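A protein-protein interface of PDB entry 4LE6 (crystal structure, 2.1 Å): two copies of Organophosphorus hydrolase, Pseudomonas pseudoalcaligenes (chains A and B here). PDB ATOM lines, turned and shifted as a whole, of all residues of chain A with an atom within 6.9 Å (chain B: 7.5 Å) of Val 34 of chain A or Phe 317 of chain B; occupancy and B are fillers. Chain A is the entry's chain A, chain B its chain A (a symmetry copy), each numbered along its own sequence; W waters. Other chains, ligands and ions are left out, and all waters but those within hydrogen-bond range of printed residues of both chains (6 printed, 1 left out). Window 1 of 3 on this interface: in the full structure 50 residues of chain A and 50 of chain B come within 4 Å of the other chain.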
ATOM      1  N   LYS A  31      -7.390   7.959 -12.399  1.00  0.00           N
ATOM      2  CA  LYS A  31      -7.871   7.955 -11.012  1.00  0.00           C
ATOM      3  C   LYS A  31      -6.725   7.728 -10.020  1.00  0.00           C
ATOM      4  O   LYS A  31      -6.463   8.561  -9.147  1.00  0.00           O
ATOM      5  CB  LYS A  31      -8.972   6.905 -10.805  1.00  0.00           C
ATOM      6  CG  LYS A  31     -10.316   7.487 -10.426  1.00  0.00           C
ATOM      7  CD  LYS A  31     -11.008   8.097 -11.630  1.00  0.00           C
ATOM      8  CE  LYS A  31     -12.162   8.989 -11.206  1.00  0.00           C
ATOM      9  NZ  LYS A  31     -12.736   9.732 -12.357  1.00  0.00           N
ATOM     10  N   THR A  32      -6.028   6.613 -10.180  1.00  0.00           N
ATOM     11  CA  THR A  32      -5.067   6.145  -9.188  1.00  0.00           C
ATOM     12  C   THR A  32      -4.075   7.234  -8.743  1.00  0.00           C
ATOM     13  O   THR A  32      -3.627   8.056  -9.553  1.00  0.00           O
ATOM     14  CB  THR A  32      -4.268   5.020  -9.796  1.00  0.00           C
ATOM     15  OG1 THR A  32      -3.642   5.524 -10.977  1.00  0.00           O
ATOM     16  CG2 THR A  32      -5.184   3.857 -10.179  1.00  0.00           C
ATOM     17  N   GLN A  33      -3.738   7.234  -7.463  1.00  0.00           N
ATOM     18  CA  GLN A  33      -2.727   8.139  -6.942  1.00  0.00           C
ATOM     19  C   GLN A  33      -1.327   7.513  -7.038  1.00  0.00           C
ATOM     20  O   GLN A  33      -1.175   6.284  -7.037  1.00  0.00           O
ATOM     21  CB  GLN A  33      -3.052   8.498  -5.493  1.00  0.00           C
ATOM     22  CG  GLN A  33      -2.139   9.574  -4.915  1.00  0.00           C
ATOM     23  CD  GLN A  33      -2.159  10.863  -5.740  1.00  0.00           C
ATOM     24  OE1 GLN A  33      -1.491  10.960  -6.766  1.00  0.00           O
ATOM     25  NE2 GLN A  33      -2.940  11.843  -5.303  1.00  0.00           N
ATOM     26  N   VAL A  34      -0.304   8.359  -7.117  1.00  0.00           N
ATOM     27  CA  VAL A  34       1.079   7.912  -7.006  1.00  0.00           C
ATOM     28  C   VAL A  34       1.198   7.088  -5.710  1.00  0.00           C
ATOM     29  O   VAL A  34       0.467   7.349  -4.761  1.00  0.00           O
ATOM     30  CB  VAL A  34       2.038   9.134  -6.954  1.00  0.00           C
ATOM     31  CG1 VAL A  34       1.866   9.904  -5.662  1.00  0.00           C
ATOM     32  CG2 VAL A  34       3.473   8.710  -7.103  1.00  0.00           C
ATOM     33  N   PRO A  35       2.086   6.073  -5.674  1.00  0.00           N
ATOM     34  CA  PRO A  35       2.243   5.309  -4.431  1.00  0.00           C
ATOM     35  C   PRO A  35       2.635   6.192  -3.242  1.00  0.00           C
ATOM     36  O   PRO A  35       3.299   7.214  -3.430  1.00  0.00           O
ATOM     37  CB  PRO A  35       3.362   4.322  -4.769  1.00  0.00           C
ATOM     38  CG  PRO A  35       3.175   4.069  -6.275  1.00  0.00           C
ATOM     39  CD  PRO A  35       2.728   5.409  -6.831  1.00  0.00           C
ATOM     40  N   GLY A  36       2.198   5.814  -2.044  1.00  0.00           N
ATOM     41  CA  GLY A  36       2.400   6.609  -0.848  1.00  0.00           C
ATOM     42  C   GLY A  36       3.717   6.267  -0.164  1.00  0.00           C
ATOM     43  O   GLY A  36       3.750   5.830   0.992  1.00  0.00           O
ATOM     44  N   TYR A  37       4.812   6.469  -0.880  1.00  0.00           N
ATOM     45  CA  TYR A  37       6.118   6.465  -0.253  1.00  0.00           C
ATOM     46  C   TYR A  37       6.949   7.637  -0.703  1.00  0.00           C
ATOM     47  O   TYR A  37       6.764   8.165  -1.808  1.00  0.00           O
ATOM     48  CB  TYR A  37       6.873   5.143  -0.472  1.00  0.00           C
ATOM     49  CG  TYR A  37       7.358   4.877  -1.884  1.00  0.00           C
ATOM     50  CD1 TYR A  37       6.553   4.214  -2.800  1.00  0.00           C
ATOM     51  CD2 TYR A  37       8.636   5.246  -2.284  1.00  0.00           C
ATOM     52  CE1 TYR A  37       6.996   3.947  -4.075  1.00  0.00           C
ATOM     53  CE2 TYR A  37       9.087   4.986  -3.561  1.00  0.00           C
ATOM     54  CZ  TYR A  37       8.263   4.349  -4.454  1.00  0.00           C
ATOM     55  OH  TYR A  37       8.713   4.087  -5.727  1.00  0.00           O
ATOM     56  N   TYR A  51       2.703   5.967   3.643  1.00  0.00           N
ATOM     57  CA  TYR A  51       1.341   6.444   3.865  1.00  0.00           C
ATOM     58  C   TYR A  51       0.435   5.274   4.199  1.00  0.00           C
ATOM     59  O   TYR A  51       0.458   4.270   3.500  1.00  0.00           O
ATOM     60  CB  TYR A  51       0.876   7.117   2.587  1.00  0.00           C
ATOM     61  CG  TYR A  51      -0.470   7.788   2.604  1.00  0.00           C
ATOM     62  CD1 TYR A  51      -0.736   8.867   3.448  1.00  0.00           C
ATOM     63  CD2 TYR A  51      -1.472   7.386   1.721  1.00  0.00           C
ATOM     64  CE1 TYR A  51      -1.985   9.501   3.423  1.00  0.00           C
ATOM     65  CE2 TYR A  51      -2.709   8.028   1.692  1.00  0.00           C
ATOM     66  CZ  TYR A  51      -2.954   9.075   2.538  1.00  0.00           C
ATOM     67  OH  TYR A  51      -4.192   9.693   2.491  1.00  0.00           O
ATOM     68  N   TYR A  54      -6.043   7.626   5.203  1.00  0.00           N
ATOM     69  CA  TYR A  54      -6.572   8.755   5.963  1.00  0.00           C
ATOM     70  C   TYR A  54      -7.782   8.355   6.781  1.00  0.00           C
ATOM     71  O   TYR A  54      -8.420   7.339   6.519  1.00  0.00           O
ATOM     72  CB  TYR A  54      -6.982   9.903   5.029  1.00  0.00           C
ATOM     73  CG  TYR A  54      -8.079   9.516   4.047  1.00  0.00           C
ATOM     74  CD1 TYR A  54      -9.430   9.651   4.374  1.00  0.00           C
ATOM     75  CD2 TYR A  54      -7.769   8.983   2.807  1.00  0.00           C
ATOM     76  CE1 TYR A  54     -10.423   9.278   3.490  1.00  0.00           C
ATOM     77  CE2 TYR A  54      -8.773   8.624   1.904  1.00  0.00           C
ATOM     78  CZ  TYR A  54     -10.089   8.773   2.258  1.00  0.00           C
ATOM     79  OH  TYR A  54     -11.082   8.415   1.373  1.00  0.00           O
ATOM     80  N   GLN A  86      -9.888  15.579   7.137  1.00  0.00           N
ATOM     81  CA  GLN A  86      -9.207  14.421   6.581  1.00  0.00           C
ATOM     82  C   GLN A  86      -7.789  14.388   7.109  1.00  0.00           C
ATOM     83  O   GLN A  86      -6.998  15.284   6.818  1.00  0.00           O
ATOM     84  CB  GLN A  86      -9.183  14.490   5.061  1.00  0.00           C
ATOM     85  CG  GLN A  86      -8.420  13.333   4.413  1.00  0.00           C
ATOM     86  CD  GLN A  86      -8.542  13.375   2.902  1.00  0.00           C
ATOM     87  OE1 GLN A  86      -9.407  14.061   2.365  1.00  0.00           O
ATOM     88  NE2 GLN A  86      -7.665  12.682   2.217  1.00  0.00           N
ATOM     89  N   ALA A  88      -4.159  12.368   7.768  1.00  0.00           N
ATOM     90  CA  ALA A  88      -3.217  11.368   7.285  1.00  0.00           C
ATOM     91  C   ALA A  88      -2.737  10.526   8.444  1.00  0.00           C
ATOM     92  O   ALA A  88      -2.716  10.992   9.594  1.00  0.00           O
ATOM     93  CB  ALA A  88      -2.022  12.054   6.646  1.00  0.00           C
ATOM     94  N   ASN A 121       2.632   0.125   0.556  1.00  0.00           N
ATOM     95  CA  ASN A 121       3.595   1.148   0.193  1.00  0.00           C
ATOM     96  C   ASN A 121       5.024   0.757   0.546  1.00  0.00           C
ATOM     97  O   ASN A 121       5.968   1.152  -0.139  1.00  0.00           O
ATOM     98  CB  ASN A 121       3.217   2.488   0.814  1.00  0.00           C
ATOM     99  CG  ASN A 121       2.044   3.134   0.093  1.00  0.00           C
ATOM    100  OD1 ASN A 121       1.987   3.134  -1.143  1.00  0.00           O
ATOM    101  ND2 ASN A 121       1.087   3.640   0.851  1.00  0.00           N
ATOM    102  N   PRO A 296       0.621  16.145   7.192  1.00  0.00           N
ATOM    103  CA  PRO A 296       0.345  15.842   5.782  1.00  0.00           C
ATOM    104  C   PRO A 296       1.497  15.065   5.169  1.00  0.00           C
ATOM    105  O   PRO A 296       2.656  15.436   5.342  1.00  0.00           O
ATOM    106  CB  PRO A 296       0.183  17.220   5.156  1.00  0.00           C
ATOM    107  CG  PRO A 296      -0.235  18.105   6.293  1.00  0.00           C
ATOM    108  CD  PRO A 296       0.554  17.592   7.451  1.00  0.00           C
ATOM    109  N   PHE A 297       1.174  13.944   4.538  1.00  0.00           N
ATOM    110  CA  PHE A 297       2.185  13.013   4.052  1.00  0.00           C
ATOM    111  C   PHE A 297       3.082  13.749   3.066  1.00  0.00           C
ATOM    112  O   PHE A 297       2.572  14.549   2.271  1.00  0.00           O
ATOM    113  CB  PHE A 297       1.493  11.836   3.348  1.00  0.00           C
ATOM    114  CG  PHE A 297       2.443  10.880   2.751  1.00  0.00           C
ATOM    115  CD1 PHE A 297       3.007   9.885   3.526  1.00  0.00           C
ATOM    116  CD2 PHE A 297       2.819  10.996   1.420  1.00  0.00           C
ATOM    117  CE1 PHE A 297       3.933   9.012   2.989  1.00  0.00           C
ATOM    118  CE2 PHE A 297       3.741  10.125   0.881  1.00  0.00           C
ATOM    119  CZ  PHE A 297       4.299   9.130   1.673  1.00  0.00           C
ATOM    120  N   PRO A 298       4.394  13.455   3.060  1.00  0.00           N
ATOM    121  CA  PRO A 298       5.188  12.455   3.784  1.00  0.00           C
ATOM    122  C   PRO A 298       5.422  12.749   5.275  1.00  0.00           C
ATOM    123  O   PRO A 298       6.045  11.951   5.966  1.00  0.00           O
ATOM    124  CB  PRO A 298       6.521  12.458   3.027  1.00  0.00           C
ATOM    125  CG  PRO A 298       6.632  13.803   2.471  1.00  0.00           C
ATOM    126  CD  PRO A 298       5.229  14.217   2.111  1.00  0.00           C
ATOM    127  N   VAL B  34      10.191   8.037  -5.224  1.00  0.00           N
ATOM    128  CA  VAL B  34       8.863   7.767  -5.760  1.00  0.00           C
ATOM    129  C   VAL B  34       8.751   8.496  -7.112  1.00  0.00           C
ATOM    130  O   VAL B  34       9.383   9.531  -7.292  1.00  0.00           O
ATOM    131  CB  VAL B  34       7.771   8.283  -4.781  1.00  0.00           C
ATOM    132  CG1 VAL B  34       7.769   9.795  -4.719  1.00  0.00           C
ATOM    133  CG2 VAL B  34       6.406   7.791  -5.175  1.00  0.00           C
ATOM    134  N   PRO B  35       7.982   7.948  -8.076  1.00  0.00           N
ATOM    135  CA  PRO B  35       7.829   8.655  -9.353  1.00  0.00           C
ATOM    136  C   PRO B  35       7.262  10.068  -9.179  1.00  0.00           C
ATOM    137  O   PRO B  35       6.502  10.312  -8.240  1.00  0.00           O
ATOM    138  CB  PRO B  35       6.854   7.767 -10.127  1.00  0.00           C
ATOM    139  CG  PRO B  35       7.168   6.352  -9.610  1.00  0.00           C
ATOM    140  CD  PRO B  35       7.498   6.550  -8.141  1.00  0.00           C
ATOM    141  N   GLY B  36       7.659  10.985 -10.058  1.00  0.00           N
ATOM    142  CA  GLY B  36       7.288  12.384  -9.952  1.00  0.00           C
ATOM    143  C   GLY B  36       5.976  12.671 -10.668  1.00  0.00           C
ATOM    144  O   GLY B  36       5.915  13.470 -11.609  1.00  0.00           O
ATOM    145  N   TYR B  37       4.915  12.018 -10.221  1.00  0.00           N
ATOM    146  CA  TYR B  37       3.579  12.417 -10.613  1.00  0.00           C
ATOM    147  C   TYR B  37       2.654  12.485  -9.427  1.00  0.00           C
ATOM    148  O   TYR B  37       2.851  11.789  -8.421  1.00  0.00           O
ATOM    149  CB  TYR B  37       2.994  11.515 -11.713  1.00  0.00           C
ATOM    150  CG  TYR B  37       2.638  10.101 -11.298  1.00  0.00           C
ATOM    151  CD1 TYR B  37       3.571   9.077 -11.382  1.00  0.00           C
ATOM    152  CD2 TYR B  37       1.356   9.782 -10.868  1.00  0.00           C
ATOM    153  CE1 TYR B  37       3.247   7.787 -11.031  1.00  0.00           C
ATOM    154  CE2 TYR B  37       1.022   8.493 -10.511  1.00  0.00           C
ATOM    155  CZ  TYR B  37       1.970   7.504 -10.582  1.00  0.00           C
ATOM    156  OH  TYR B  37       1.639   6.216 -10.228  1.00  0.00           O
ATOM    157  N   TYR B  38       1.653  13.347  -9.544  1.00  0.00           N
ATOM    158  CA  TYR B  38       0.675  13.502  -8.473  1.00  0.00           C
ATOM    159  C   TYR B  38      -0.716  13.797  -9.028  1.00  0.00           C
ATOM    160  O   TYR B  38      -0.874  14.723  -9.815  1.00  0.00           O
ATOM    161  CB  TYR B  38       1.087  14.637  -7.521  1.00  0.00           C
ATOM    162  CG  TYR B  38       0.117  14.790  -6.390  1.00  0.00           C
ATOM    163  CD1 TYR B  38       0.146  13.912  -5.322  1.00  0.00           C
ATOM    164  CD2 TYR B  38      -0.860  15.786  -6.393  1.00  0.00           C
ATOM    165  CE1 TYR B  38      -0.748  14.016  -4.285  1.00  0.00           C
ATOM    166  CE2 TYR B  38      -1.767  15.894  -5.345  1.00  0.00           C
ATOM    167  CZ  TYR B  38      -1.697  14.996  -4.288  1.00  0.00           C
ATOM    168  OH  TYR B  38      -2.560  15.034  -3.203  1.00  0.00           O
ATOM    169  N   ARG B  39      -1.718  13.030  -8.587  1.00  0.00           N
ATOM    170  CA  ARG B  39      -3.085  13.158  -9.095  1.00  0.00           C
ATOM    171  C   ARG B  39      -3.971  14.039  -8.205  1.00  0.00           C
ATOM    172  O   ARG B  39      -3.947  13.914  -6.980  1.00  0.00           O
ATOM    173  CB  ARG B  39      -3.725  11.781  -9.187  1.00  0.00           C
ATOM    174  CG  ARG B  39      -4.785  11.668 -10.267  1.00  0.00           C
ATOM    175  CD  ARG B  39      -4.165  11.289 -11.595  1.00  0.00           C
ATOM    176  NE  ARG B  39      -3.644   9.931 -11.560  1.00  0.00           N
ATOM    177  CZ  ARG B  39      -2.815   9.415 -12.460  1.00  0.00           C
ATOM    178  NH1 ARG B  39      -2.415   8.160 -12.337  1.00  0.00           N
ATOM    179  NH2 ARG B  39      -2.386  10.142 -13.483  1.00  0.00           N
ATOM    180  N   ALA B 124       4.753   7.019 -16.285  1.00  0.00           N
ATOM    181  CA  ALA B 124       4.583   6.399 -14.969  1.00  0.00           C
ATOM    182  C   ALA B 124       3.179   6.644 -14.427  1.00  0.00           C
ATOM    183  O   ALA B 124       2.603   5.798 -13.741  1.00  0.00           O
ATOM    184  CB  ALA B 124       5.631   6.933 -13.987  1.00  0.00           C
ATOM    185  N   SER B 125       2.611   7.796 -14.765  1.00  0.00           N
ATOM    186  CA  SER B 125       1.283   8.154 -14.285  1.00  0.00           C
ATOM    187  C   SER B 125       0.161   7.403 -15.025  1.00  0.00           C
ATOM    188  O   SER B 125      -1.018   7.548 -14.691  1.00  0.00           O
ATOM    189  CB  SER B 125       1.069   9.662 -14.414  1.00  0.00           C
ATOM    190  OG  SER B 125       0.632  10.011 -15.704  1.00  0.00           O
ATOM    191  N   PHE B 297       7.320  20.697  -6.055  1.00  0.00           N
ATOM    192  CA  PHE B 297       6.455  19.718  -6.702  1.00  0.00           C
ATOM    193  C   PHE B 297       5.549  19.104  -5.644  1.00  0.00           C
ATOM    194  O   PHE B 297       6.017  18.845  -4.528  1.00  0.00           O
ATOM    195  CB  PHE B 297       7.320  18.624  -7.346  1.00  0.00           C
ATOM    196  CG  PHE B 297       6.526  17.543  -7.957  1.00  0.00           C
ATOM    197  CD1 PHE B 297       6.026  17.687  -9.237  1.00  0.00           C
ATOM    198  CD2 PHE B 297       6.228  16.394  -7.239  1.00  0.00           C
ATOM    199  CE1 PHE B 297       5.243  16.701  -9.803  1.00  0.00           C
ATOM    200  CE2 PHE B 297       5.449  15.406  -7.803  1.00  0.00           C
ATOM    201  CZ  PHE B 297       4.954  15.565  -9.090  1.00  0.00           C
ATOM    202  N   PRO B 298       4.281  18.812  -5.985  1.00  0.00           N
ATOM    203  CA  PRO B 298       3.558  18.883  -7.262  1.00  0.00           C
ATOM    204  C   PRO B 298       3.194  20.298  -7.738  1.00  0.00           C
ATOM    205  O   PRO B 298       2.620  20.454  -8.810  1.00  0.00           O
ATOM    206  CB  PRO B 298       2.286  18.073  -6.983  1.00  0.00           C
ATOM    207  CG  PRO B 298       2.063  18.211  -5.547  1.00  0.00           C
ATOM    208  CD  PRO B 298       3.431  18.250  -4.918  1.00  0.00           C
ATOM    209  N   PRO B 314       0.452  24.608   0.071  1.00  0.00           N
ATOM    210  CA  PRO B 314       0.454  23.444  -0.821  1.00  0.00           C
ATOM    211  C   PRO B 314      -0.663  22.477  -0.474  1.00  0.00           C
ATOM    212  O   PRO B 314      -1.054  22.364   0.687  1.00  0.00           O
ATOM    213  CB  PRO B 314       1.812  22.797  -0.558  1.00  0.00           C
ATOM    214  CG  PRO B 314       2.183  23.237   0.855  1.00  0.00           C
ATOM    215  CD  PRO B 314       1.546  24.572   1.059  1.00  0.00           C
ATOM    216  N   VAL B 315      -1.174  21.788  -1.483  1.00  0.00           N
ATOM    217  CA  VAL B 315      -2.185  20.777  -1.264  1.00  0.00           C
ATOM    218  C   VAL B 315      -1.630  19.691  -0.350  1.00  0.00           C
ATOM    219  O   VAL B 315      -0.420  19.402  -0.344  1.00  0.00           O
ATOM    220  CB  VAL B 315      -2.634  20.159  -2.602  1.00  0.00           C
ATOM    221  CG1 VAL B 315      -1.507  19.382  -3.219  1.00  0.00           C
ATOM    222  CG2 VAL B 315      -3.865  19.296  -2.418  1.00  0.00           C
ATOM    223  N   GLU B 316      -2.517  19.092   0.427  1.00  0.00           N
ATOM    224  CA  GLU B 316      -2.141  17.980   1.280  1.00  0.00           C
ATOM    225  C   GLU B 316      -2.333  16.675   0.521  1.00  0.00           C
ATOM    226  O   GLU B 316      -3.380  16.453  -0.076  1.00  0.00           O
ATOM    227  CB  GLU B 316      -2.972  18.003   2.563  1.00  0.00           C
ATOM    228  CG  GLU B 316      -2.711  19.260   3.396  1.00  0.00           C
ATOM    229  CD  GLU B 316      -3.526  19.328   4.672  1.00  0.00           C
ATOM    230  OE1 GLU B 316      -3.706  18.281   5.330  1.00  0.00           O
ATOM    231  OE2 GLU B 316      -3.999  20.438   5.020  1.00  0.00           O
ATOM    232  N   PHE B 317      -1.317  15.814   0.553  1.00  0.00           N
ATOM    233  CA  PHE B 317      -1.365  14.540  -0.140  1.00  0.00           C
ATOM    234  C   PHE B 317      -2.663  13.780   0.167  1.00  0.00           C
ATOM    235  O   PHE B 317      -3.042  13.618   1.338  1.00  0.00           O
ATOM    236  CB  PHE B 317      -0.162  13.710   0.282  1.00  0.00           C
ATOM    237  CG  PHE B 317      -0.007  12.437  -0.494  1.00  0.00           C
ATOM    238  CD1 PHE B 317      -0.695  11.297  -0.128  1.00  0.00           C
ATOM    239  CD2 PHE B 317       0.848  12.378  -1.578  1.00  0.00           C
ATOM    240  CE1 PHE B 317      -0.545  10.125  -0.838  1.00  0.00           C
ATOM    241  CE2 PHE B 317       0.992  11.204  -2.298  1.00  0.00           C
ATOM    242  CZ  PHE B 317       0.295  10.081  -1.926  1.00  0.00           C
ATOM    243  N   SER B 318      -3.345  13.322  -0.880  1.00  0.00           N
ATOM    244  CA  SER B 318      -4.617  12.628  -0.730  1.00  0.00           C
ATOM    245  C   SER B 318      -4.898  11.763  -1.938  1.00  0.00           C
ATOM    246  O   SER B 318      -4.609  12.151  -3.064  1.00  0.00           O
ATOM    247  CB  SER B 318      -5.765  13.635  -0.606  1.00  0.00           C
ATOM    248  OG  SER B 318      -7.020  12.973  -0.546  1.00  0.00           O
ATOM    249  N   PRO B 319      -5.498  10.594  -1.719  1.00  0.00           N
ATOM    250  CA  PRO B 319      -6.066   9.955  -2.909  1.00  0.00           C
ATOM    251  C   PRO B 319      -7.232  10.768  -3.448  1.00  0.00           C
ATOM    252  O   PRO B 319      -7.761  11.659  -2.775  1.00  0.00           O
ATOM    253  CB  PRO B 319      -6.552   8.594  -2.395  1.00  0.00           C
ATOM    254  CG  PRO B 319      -6.619   8.717  -0.905  1.00  0.00           C
ATOM    255  CD  PRO B 319      -5.658   9.789  -0.500  1.00  0.00           C
HETATM  256  O   HOH W   1      -2.414   4.852 -13.272  1.00  0.00           O
HETATM  257  O   HOH W   2      -8.847  15.342  -0.139  1.00  0.00           O
HETATM  258  O   HOH W   3      -0.772   5.167  -9.704  1.00  0.00           O
HETATM  259  O   HOH W   4      -1.628  14.012   3.666  1.00  0.00           O
HETATM  260  O   HOH W   5      -4.635  12.232   3.212  1.00  0.00           O
HETATM  261  O   HOH W   6       0.939  16.600   1.991  1.00  0.00           O
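The guanidinium group of Arg 39 of chain B sits at hydrogen-bond distance from the backbone carbonyl oxygen of Thr 32 of chain A (2.7 Å). The side-chain amide oxygen (OE1) of Gln 33 of chain A is in hydrogen-bond range of the backbone NH (N) of Arg 39 of chain B (2.8 Å). NE2 of Gln 33 of chain A sits at hydrogen-bond distance from O of Ser 318 of chain B (2.8 Å). The side-chain hydroxyl (OG) of Ser 318 of chain B lies within hydrogen-bond range of the side-chain amide nitrogen (NE2) of Gln 86 of chain A, 2.9 Å away.
N of Tyr 51 of chain A lies within hydrogen-bond range of O of Gly 36 of chain A (2.9 Å). The backbone carbonyl oxygen of Tyr 51 of chain A is in hydrogen-bond range of the side-chain amide nitrogen of Asn 121 of chain A. The side-chain hydroxyl (OH) of Tyr 38 of chain B sits at hydrogen-bond distance from the backbone NH (N) of Ser 318 of chain B (3.0 Å). The backbone carbonyl oxygen (O) of Ser 125 of chain B is in hydrogen-bond range of the guanidinium group (NH1) of Arg 39 of chain B (2.8 Å).
O of Lys 31 of chain A touches CG of Arg 39 of chain B, at 3.7 Å. CG of Gln 33 of chain A touches CZ of Phe 317 of chain B (3.9 Å). Val 34 of chain A touches Val 34 of chain B. Phe 317 of chain B touches Val 34 of chain A (CE2 to CG1, 3.7 Å). Pro 35 of chain A touches Val 34 of chain B (O to CG2, 3.6 Å). O of Tyr 37 of chain A touches CB of Val 34 of chain B (3.1 Å). Pro 35 of chain B touches Tyr 37 of chain A (CD to OH, 3.7 Å). Tyr 51 of chain A touches Pro 319 of chain B (OH to CD, 3.3 Å). CE2 of Tyr 54 of chain A touches CG of Pro 319 of chain B, at 3.5 Å. CG of Pro 296 of chain A touches OE1 of Glu 316 of chain B, at 3.6 Å.
Of the printed residues of chain B, Val 34 of chain A touches Val 34, Pro 35, Tyr 37 and Phe 317. Of chain A, only Gln 33 (3.9 Å), Val 34 (3.7 Å), Tyr 51 (3.9 Å) and Phe 297 (3.5 Å) come within 4 Å of Phe 317 of chain B. Of the printed residues of chain B, Pro 35 of chain A touches Val 34 and Tyr 37. Of the printed residues of chain B, Tyr 51 of chain A touches Phe 317 and Pro 319. Of the printed residues of chain B, Lys 31 of chain A touches Arg 39. The nearest residue of chain B that does not touch Val 34 of chain A is Tyr 38 of chain B (4.4 Å). The nearest residue of chain A that does not touch Phe 317 of chain B is Gly 36 of chain A (4.2 Å). The nearest printed residue of chain B that does not touch Pro 35 of chain A is Phe 317 of chain B (4.4 Å).
Of the 16 printed residues of chain B, 9 touch a printed residue of chain A. Hydrophobic or aromatic side chains of chain B that line the printed part of chain A: Val 34, Pro 35, Tyr 37, Tyr 38, Phe 317 and Pro 319.
Val 34 of chain B touches its own counterpart, Val 34 of chain A. Val 34 of chain A touches Pro 35 of chain B, and with the chains exchanged Pro 35 of chain A touches Val 34 of chain B. Val 34 of chain A touches Tyr 37 of chain B, and with the chains exchanged Tyr 37 of chain A touches Val 34 of chain B. Pro 35 of chain A touches Tyr 37 of chain B, and with the chains exchanged Tyr 37 of chain A touches Pro 35 of chain B.
Water W6 bridges O of Phe 297 of chain A and N of Phe 317 of chain B. Water W5 lies within hydrogen-bond range of OH of Tyr 51 of chain A, O of Phe 317 of chain B and NE2 of Gln 86 of chain A. Water W3 lies within hydrogen-bond range of OH of Tyr 37 of chain B (2.7 Å), O of Gln 33 of chain A (2.9 Å) and OG1 of Thr 32 of chain A (3.2 Å). Water W1 lies within hydrogen-bond range of OG1 of Thr 32 of chain A, O of Ser 125 of chain B and NH1 of Arg 39 of chain B. Water W4 lies within hydrogen-bond range of the backbone carbonyl oxygen (O) of Phe 317 of chain B (2.8 Å) and the backbone NH (N) of Phe 297 of chain A (2.9 Å). Water W2 bridges OE1 of Gln 86 of chain A (2.9 Å) and OG of Ser 318 of chain B (3.0 Å).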
